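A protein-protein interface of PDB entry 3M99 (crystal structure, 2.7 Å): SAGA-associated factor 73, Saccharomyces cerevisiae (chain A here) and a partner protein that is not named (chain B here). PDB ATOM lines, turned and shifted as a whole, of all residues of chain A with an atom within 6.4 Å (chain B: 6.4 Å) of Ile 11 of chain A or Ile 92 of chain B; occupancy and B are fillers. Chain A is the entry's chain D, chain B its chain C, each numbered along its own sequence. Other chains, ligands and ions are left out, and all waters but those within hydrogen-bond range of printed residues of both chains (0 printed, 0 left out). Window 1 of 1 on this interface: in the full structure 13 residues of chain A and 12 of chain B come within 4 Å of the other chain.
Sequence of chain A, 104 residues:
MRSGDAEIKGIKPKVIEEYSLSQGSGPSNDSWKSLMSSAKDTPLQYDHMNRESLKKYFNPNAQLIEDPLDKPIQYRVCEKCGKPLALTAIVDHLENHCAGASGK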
ATOM      1  N   LYS A   9      -4.997 -20.252  -2.128  1.00  0.00           N
ATOM      2  CA  LYS A   9      -5.343 -18.897  -1.713  1.00  0.00           C
ATOM      3  C   LYS A   9      -4.347 -18.356  -0.686  1.00  0.00           C
ATOM      4  O   LYS A   9      -4.471 -18.623   0.508  1.00  0.00           O
ATOM      5  CB  LYS A   9      -6.771 -18.853  -1.154  1.00  0.00           C
ATOM      6  CG  LYS A   9      -7.367 -17.449  -1.055  1.00  0.00           C
ATOM      7  CD  LYS A   9      -8.894 -17.475  -0.965  1.00  0.00           C
ATOM      8  CE  LYS A   9      -9.384 -17.844   0.431  1.00  0.00           C
ATOM      9  NZ  LYS A   9      -9.169 -19.280   0.765  1.00  0.00           N
ATOM     10  N   GLY A  10      -3.362 -17.598  -1.161  1.00  0.00           N
ATOM     11  CA  GLY A  10      -2.357 -17.002  -0.295  1.00  0.00           C
ATOM     12  C   GLY A  10      -0.957 -17.562  -0.487  1.00  0.00           C
ATOM     13  O   GLY A  10      -0.773 -18.772  -0.616  1.00  0.00           O
ATOM     14  N   ILE A  11       0.035 -16.674  -0.506  1.00  0.00           N
ATOM     15  CA  ILE A  11       1.435 -17.075  -0.628  1.00  0.00           C
ATOM     16  C   ILE A  11       2.127 -17.091   0.735  1.00  0.00           C
ATOM     17  O   ILE A  11       2.215 -16.065   1.411  1.00  0.00           O
ATOM     18  CB  ILE A  11       2.213 -16.142  -1.572  1.00  0.00           C
ATOM     19  CG1 ILE A  11       3.699 -16.501  -1.570  1.00  0.00           C
ATOM     20  CG2 ILE A  11       2.017 -14.686  -1.167  1.00  0.00           C
ATOM     21  CD1 ILE A  11       4.539 -15.617  -2.464  1.00  0.00           C
ATOM     22  N   LYS A  12       2.621 -18.262   1.125  1.00  0.00           N
ATOM     23  CA  LYS A  12       3.240 -18.450   2.435  1.00  0.00           C
ATOM     24  C   LYS A  12       4.061 -17.235   2.865  1.00  0.00           C
ATOM     25  O   LYS A  12       4.952 -16.793   2.139  1.00  0.00           O
ATOM     26  CB  LYS A  12       4.105 -19.712   2.429  1.00  0.00           C
ATOM     27  CG  LYS A  12       4.232 -20.405   3.778  1.00  0.00           C
ATOM     28  CD  LYS A  12       4.404 -21.908   3.598  1.00  0.00           C
ATOM     29  CE  LYS A  12       3.221 -22.502   2.838  1.00  0.00           C
ATOM     30  NZ  LYS A  12       3.355 -23.967   2.611  1.00  0.00           N
ATOM     31  N   PRO A  13       3.745 -16.686   4.049  1.00  0.00           N
ATOM     32  CA  PRO A  13       4.346 -15.475   4.629  1.00  0.00           C
ATOM     33  C   PRO A  13       5.865 -15.535   4.830  1.00  0.00           C
ATOM     34  O   PRO A  13       6.523 -14.501   4.705  1.00  0.00           O
ATOM     35  CB  PRO A  13       3.636 -15.347   5.981  1.00  0.00           C
ATOM     36  CG  PRO A  13       2.325 -16.024   5.775  1.00  0.00           C
ATOM     37  CD  PRO A  13       2.618 -17.179   4.860  1.00  0.00           C
ATOM     38  N   LYS A  14       6.408 -16.707   5.147  1.00  0.00           N
ATOM     39  CA  LYS A  14       7.855 -16.855   5.298  1.00  0.00           C
ATOM     40  C   LYS A  14       8.548 -16.816   3.941  1.00  0.00           C
ATOM     41  O   LYS A  14       9.685 -16.358   3.823  1.00  0.00           O
ATOM     42  CB  LYS A  14       8.199 -18.157   6.020  1.00  0.00           C
ATOM     43  CG  LYS A  14       9.618 -18.645   5.752  1.00  0.00           C
ATOM     44  CD  LYS A  14      10.662 -17.647   6.239  1.00  0.00           C
ATOM     45  CE  LYS A  14      12.017 -17.909   5.596  1.00  0.00           C
ATOM     46  NZ  LYS A  14      11.948 -17.829   4.109  1.00  0.00           N
ATOM     47  N   VAL A  15       7.854 -17.308   2.920  1.00  0.00           N
ATOM     48  CA  VAL A  15       8.368 -17.289   1.559  1.00  0.00           C
ATOM     49  C   VAL A  15       8.459 -15.854   1.049  1.00  0.00           C
ATOM     50  O   VAL A  15       9.472 -15.454   0.476  1.00  0.00           O
ATOM     51  CB  VAL A  15       7.478 -18.116   0.621  1.00  0.00           C
ATOM     52  CG1 VAL A  15       8.022 -18.074  -0.796  1.00  0.00           C
ATOM     53  CG2 VAL A  15       7.378 -19.550   1.123  1.00  0.00           C
ATOM     54  N   ILE A  16       7.397 -15.082   1.266  1.00  0.00           N
ATOM     55  CA  ILE A  16       7.399 -13.671   0.898  1.00  0.00           C
ATOM     56  C   ILE A  16       8.451 -12.926   1.710  1.00  0.00           C
ATOM     57  O   ILE A  16       9.101 -12.016   1.210  1.00  0.00           O
ATOM     58  CB  ILE A  16       6.017 -13.005   1.114  1.00  0.00           C
ATOM     59  CG1 ILE A  16       5.806 -12.651   2.587  1.00  0.00           C
ATOM     60  CG2 ILE A  16       4.899 -13.901   0.601  1.00  0.00           C
ATOM     61  CD1 ILE A  16       4.444 -12.069   2.888  1.00  0.00           C
ATOM     62  N   SER A  20       9.762 -13.086  -2.826  1.00  0.00           N
ATOM     63  CA  SER A  20       8.577 -12.524  -3.474  1.00  0.00           C
ATOM     64  C   SER A  20       7.794 -11.545  -2.597  1.00  0.00           C
ATOM     65  O   SER A  20       6.830 -11.927  -1.930  1.00  0.00           O
ATOM     66  CB  SER A  20       7.660 -13.651  -3.950  1.00  0.00           C
ATOM     67  OG  SER A  20       7.520 -14.637  -2.944  1.00  0.00           O
ATOM     68  N   LEU B   8      -1.177 -12.832  -7.703  1.00  0.00           N
ATOM     69  CA  LEU B   8      -0.356 -13.867  -7.089  1.00  0.00           C
ATOM     70  C   LEU B   8      -0.020 -14.999  -8.058  1.00  0.00           C
ATOM     71  O   LEU B   8       0.280 -16.113  -7.636  1.00  0.00           O
ATOM     72  CB  LEU B   8      -1.060 -14.424  -5.850  1.00  0.00           C
ATOM     73  CG  LEU B   8      -1.466 -13.362  -4.823  1.00  0.00           C
ATOM     74  CD1 LEU B   8      -2.431 -13.924  -3.786  1.00  0.00           C
ATOM     75  CD2 LEU B   8      -0.231 -12.760  -4.161  1.00  0.00           C
ATOM     76  N   GLN B  11       3.947 -13.488  -8.817  1.00  0.00           N
ATOM     77  CA  GLN B  11       4.782 -13.588  -7.629  1.00  0.00           C
ATOM     78  C   GLN B  11       5.175 -15.038  -7.355  1.00  0.00           C
ATOM     79  O   GLN B  11       6.306 -15.322  -6.959  1.00  0.00           O
ATOM     80  CB  GLN B  11       4.084 -12.982  -6.408  1.00  0.00           C
ATOM     81  CG  GLN B  11       4.280 -11.482  -6.259  1.00  0.00           C
ATOM     82  CD  GLN B  11       3.875 -10.968  -4.888  1.00  0.00           C
ATOM     83  OE1 GLN B  11       4.259 -11.528  -3.858  1.00  0.00           O
ATOM     84  NE2 GLN B  11       3.102  -9.891  -4.869  1.00  0.00           N
ATOM     85  N   ILE B  12       4.238 -15.952  -7.572  1.00  0.00           N
ATOM     86  CA  ILE B  12       4.485 -17.365  -7.328  1.00  0.00           C
ATOM     87  C   ILE B  12       5.475 -17.914  -8.361  1.00  0.00           C
ATOM     88  O   ILE B  12       6.188 -18.886  -8.112  1.00  0.00           O
ATOM     89  CB  ILE B  12       3.161 -18.161  -7.328  1.00  0.00           C
ATOM     90  CG1 ILE B  12       3.390 -19.609  -6.893  1.00  0.00           C
ATOM     91  CG2 ILE B  12       2.503 -18.109  -8.697  1.00  0.00           C
ATOM     92  CD1 ILE B  12       3.737 -20.542  -8.037  1.00  0.00           C
ATOM     93  N   GLN B  13       5.523 -17.262  -9.518  1.00  0.00           N
ATOM     94  CA  GLN B  13       6.462 -17.621 -10.569  1.00  0.00           C
ATOM     95  C   GLN B  13       7.823 -17.044 -10.199  1.00  0.00           C
ATOM     96  O   GLN B  13       8.862 -17.632 -10.485  1.00  0.00           O
ATOM     97  CB  GLN B  13       5.984 -17.034 -11.897  1.00  0.00           C
ATOM     98  CG  GLN B  13       6.101 -17.956 -13.100  1.00  0.00           C
ATOM     99  CD  GLN B  13       5.360 -17.408 -14.313  1.00  0.00           C
ATOM    100  OE1 GLN B  13       5.634 -17.784 -15.450  1.00  0.00           O
ATOM    101  NE2 GLN B  13       4.416 -16.506 -14.068  1.00  0.00           N
ATOM    102  N   TYR B  15       9.192 -16.718  -7.219  1.00  0.00           N
ATOM    103  CA  TYR B  15       9.916 -17.546  -6.262  1.00  0.00           C
ATOM    104  C   TYR B  15      10.647 -18.661  -6.984  1.00  0.00           C
ATOM    105  O   TYR B  15      11.852 -18.836  -6.811  1.00  0.00           O
ATOM    106  CB  TYR B  15       8.990 -18.153  -5.208  1.00  0.00           C
ATOM    107  CG  TYR B  15       9.676 -19.235  -4.401  1.00  0.00           C
ATOM    108  CD1 TYR B  15       9.575 -20.574  -4.765  1.00  0.00           C
ATOM    109  CD2 TYR B  15      10.453 -18.918  -3.291  1.00  0.00           C
ATOM    110  CE1 TYR B  15      10.217 -21.575  -4.036  1.00  0.00           C
ATOM    111  CE2 TYR B  15      11.100 -19.910  -2.554  1.00  0.00           C
ATOM    112  CZ  TYR B  15      10.978 -21.237  -2.931  1.00  0.00           C
ATOM    113  OH  TYR B  15      11.615 -22.221  -2.205  1.00  0.00           O
ATOM    114  N   LEU B  16       9.911 -19.417  -7.792  1.00  0.00           N
ATOM    115  CA  LEU B  16      10.495 -20.535  -8.519  1.00  0.00           C
ATOM    116  C   LEU B  16      11.841 -20.164  -9.137  1.00  0.00           C
ATOM    117  O   LEU B  16      12.799 -20.931  -9.057  1.00  0.00           O
ATOM    118  CB  LEU B  16       9.529 -21.065  -9.582  1.00  0.00           C
ATOM    119  CG  LEU B  16       8.713 -22.300  -9.194  1.00  0.00           C
ATOM    120  CD1 LEU B  16       8.117 -22.159  -7.807  1.00  0.00           C
ATOM    121  CD2 LEU B  16       7.631 -22.560 -10.214  1.00  0.00           C
ATOM    122  N   PHE B  88       6.279 -28.328  -5.657  1.00  0.00           N
ATOM    123  CA  PHE B  88       7.058 -27.110  -5.430  1.00  0.00           C
ATOM    124  C   PHE B  88       6.167 -25.962  -4.960  1.00  0.00           C
ATOM    125  O   PHE B  88       6.567 -25.150  -4.124  1.00  0.00           O
ATOM    126  CB  PHE B  88       7.810 -26.686  -6.695  1.00  0.00           C
ATOM    127  CG  PHE B  88       9.044 -27.493  -6.970  1.00  0.00           C
ATOM    128  CD1 PHE B  88       9.503 -27.654  -8.266  1.00  0.00           C
ATOM    129  CD2 PHE B  88       9.742 -28.096  -5.935  1.00  0.00           C
ATOM    130  CE1 PHE B  88      10.637 -28.390  -8.528  1.00  0.00           C
ATOM    131  CE2 PHE B  88      10.879 -28.842  -6.189  1.00  0.00           C
ATOM    132  CZ  PHE B  88      11.327 -28.988  -7.488  1.00  0.00           C
ATOM    133  N   LEU B  89       4.960 -25.894  -5.510  1.00  0.00           N
ATOM    134  CA  LEU B  89       4.016 -24.850  -5.137  1.00  0.00           C
ATOM    135  C   LEU B  89       3.641 -24.983  -3.667  1.00  0.00           C
ATOM    136  O   LEU B  89       3.490 -23.984  -2.963  1.00  0.00           O
ATOM    137  CB  LEU B  89       2.763 -24.914  -6.015  1.00  0.00           C
ATOM    138  CG  LEU B  89       2.810 -24.212  -7.377  1.00  0.00           C
ATOM    139  CD1 LEU B  89       4.105 -24.502  -8.117  1.00  0.00           C
ATOM    140  CD2 LEU B  89       1.606 -24.600  -8.226  1.00  0.00           C
ATOM    141  N   GLU B  90       3.503 -26.223  -3.206  1.00  0.00           N
ATOM    142  CA  GLU B  90       3.124 -26.488  -1.822  1.00  0.00           C
ATOM    143  C   GLU B  90       4.280 -26.176  -0.871  1.00  0.00           C
ATOM    144  O   GLU B  90       4.179 -26.368   0.340  1.00  0.00           O
ATOM    145  CB  GLU B  90       2.644 -27.935  -1.663  1.00  0.00           C
ATOM    146  CG  GLU B  90       1.635 -28.359  -2.728  1.00  0.00           C
ATOM    147  CD  GLU B  90       0.813 -29.573  -2.330  1.00  0.00           C
ATOM    148  OE1 GLU B  90      -0.011 -29.455  -1.398  1.00  0.00           O
ATOM    149  OE2 GLU B  90       0.978 -30.638  -2.966  1.00  0.00           O
ATOM    150  N   GLU B  91       5.376 -25.687  -1.439  1.00  0.00           N
ATOM    151  CA  GLU B  91       6.510 -25.233  -0.653  1.00  0.00           C
ATOM    152  C   GLU B  91       6.355 -23.753  -0.346  1.00  0.00           C
ATOM    153  O   GLU B  91       7.027 -23.217   0.535  1.00  0.00           O
ATOM    154  CB  GLU B  91       7.815 -25.457  -1.418  1.00  0.00           C
ATOM    155  CG  GLU B  91       8.111 -26.908  -1.750  1.00  0.00           C
ATOM    156  CD  GLU B  91       8.514 -27.717  -0.535  1.00  0.00           C
ATOM    157  OE1 GLU B  91       7.835 -27.615   0.511  1.00  0.00           O
ATOM    158  OE2 GLU B  91       9.510 -28.464  -0.631  1.00  0.00           O
ATOM    159  N   ILE B  92       5.468 -23.091  -1.083  1.00  0.00           N
ATOM    160  CA  ILE B  92       5.315 -21.646  -0.956  1.00  0.00           C
ATOM    161  C   ILE B  92       3.856 -21.193  -0.990  1.00  0.00           C
ATOM    162  O   ILE B  92       3.567 -20.014  -1.206  1.00  0.00           O
ATOM    163  CB  ILE B  92       6.104 -20.901  -2.055  1.00  0.00           C
ATOM    164  CG1 ILE B  92       5.545 -21.228  -3.439  1.00  0.00           C
ATOM    165  CG2 ILE B  92       7.577 -21.265  -1.991  1.00  0.00           C
ATOM    166  CD1 ILE B  92       6.248 -20.499  -4.568  1.00  0.00           C
ATOM    167  N   VAL B  93       2.937 -22.125  -0.766  1.00  0.00           N
ATOM    168  CA  VAL B  93       1.519 -21.796  -0.824  1.00  0.00           C
ATOM    169  C   VAL B  93       0.713 -22.440   0.299  1.00  0.00           C
ATOM    170  O   VAL B  93       0.730 -23.662   0.470  1.00  0.00           O
ATOM    171  CB  VAL B  93       0.902 -22.194  -2.182  1.00  0.00           C
ATOM    172  CG1 VAL B  93      -0.604 -21.963  -2.175  1.00  0.00           C
ATOM    173  CG2 VAL B  93       1.560 -21.415  -3.312  1.00  0.00           C
ATOM    174  N   ASP B  94       0.015 -21.605   1.063  1.00  0.00           N
ATOM    175  CA  ASP B  94      -0.953 -22.090   2.037  1.00  0.00           C
ATOM    176  C   ASP B  94      -2.189 -22.570   1.287  1.00  0.00           C
ATOM    177  O   ASP B  94      -2.633 -21.928   0.334  1.00  0.00           O
ATOM    178  CB  ASP B  94      -1.318 -20.990   3.038  1.00  0.00           C
ATOM    179  CG  ASP B  94      -0.242 -20.776   4.090  1.00  0.00           C
ATOM    180  OD1 ASP B  94       0.030 -21.716   4.867  1.00  0.00           O
ATOM    181  OD2 ASP B  94       0.325 -19.665   4.150  1.00  0.00           O
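Lys 9 of chain A touches Asp 94 of chain B (O to O, 3.8 Å). Val 93 of chain B touches Gly 10 of chain A (CG1 to O, 3.6 Å). Ile 11 of chain A touches Ile 92 of chain B (CG1 to O, 3.5 Å). Asp 94 of chain B touches Lys 12 of chain A (OD2 to CA, 3.6 Å). Pro 13 of chain A touches Asp 94 of chain B (CD to OD2, 3.5 Å). Val 15 of chain A touches Tyr 15 of chain B. CG2 of Val 15 of chain A touches O of Glu 91 of chain B (3.7 Å). Ile 92 of chain B touches Val 15 of chain A (CG2 to CG1, 3.4 Å).
Of the 13 printed residues of chain B, 7 touch a printed residue of chain A. Hydrophobic or aromatic side chains of chain B within 4 Å of the printed part of chain A: Tyr 15, Ile 92 and Val 93. Printed residues of chain A that touch a printed residue of chain B: Lys 9, Gly 10, Ile 11, Lys 12, Pro 13, Val 15 and Ser 20. Hydrophobic or aromatic side chains of chain A within 4 Å of the printed part of chain B: Ile 11, Pro 13 and Val 15. Among the printed residues, 13 pairs touch across the chains. Among the printed residues, no Asp or Glu carboxylate lies within 4 Å of a Lys or Arg side-chain nitrogen of the other chain.
Ile 11 of chain A touches one residue of chain B. Of chain A, only Ile 11, Lys 12 and Val 15 come within 4 Å of Ile 92 of chain B. Of the printed residues of chain B, Ser 20 of chain A touches Gln 11. Of the printed residues of chain B, Lys 12 of chain A touches Glu 90, Ile 92, Val 93 and Asp 94. Of the printed residues of chain B, Val 15 of chain A touches Tyr 15 (3.6 Å), Glu 91 (3.7 Å) and Ile 92 (3.4 Å). Lys 14 of chain A touches none of the printed residues of chain B. Leu 89 of chain B touches none of the printed residues of chain A. The nearest printed residue of chain A that does not touch Asp 94 of chain B is Ile 11 of chain A (4.6 Å).
The side-chain amide oxygen (OE1) of Gln 11 of chain B lies close to the backbone carbonyl oxygen (O) of Ser 20 of chain A, 3.2 Å away. The backbone carbonyl oxygen of Glu 90 of chain B sits at hydrogen-bond distance from the side-chain amino group of Lys 12 of chain A. The backbone carbonyl oxygen (O) of Ile 92 of chain B is in hydrogen-bond range of the backbone NH (N) of Lys 12 of chain A (3.1 Å). The backbone carbonyl oxygen of Val 93 of chain B lies within hydrogen-bond range of the side-chain amino group of Lys 12 of chain A, at 3.4 Å. The backbone NH of Asp 94 of chain B sits at hydrogen-bond distance from the backbone carbonyl oxygen of Gly 10 of chain A (3.4 Å).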
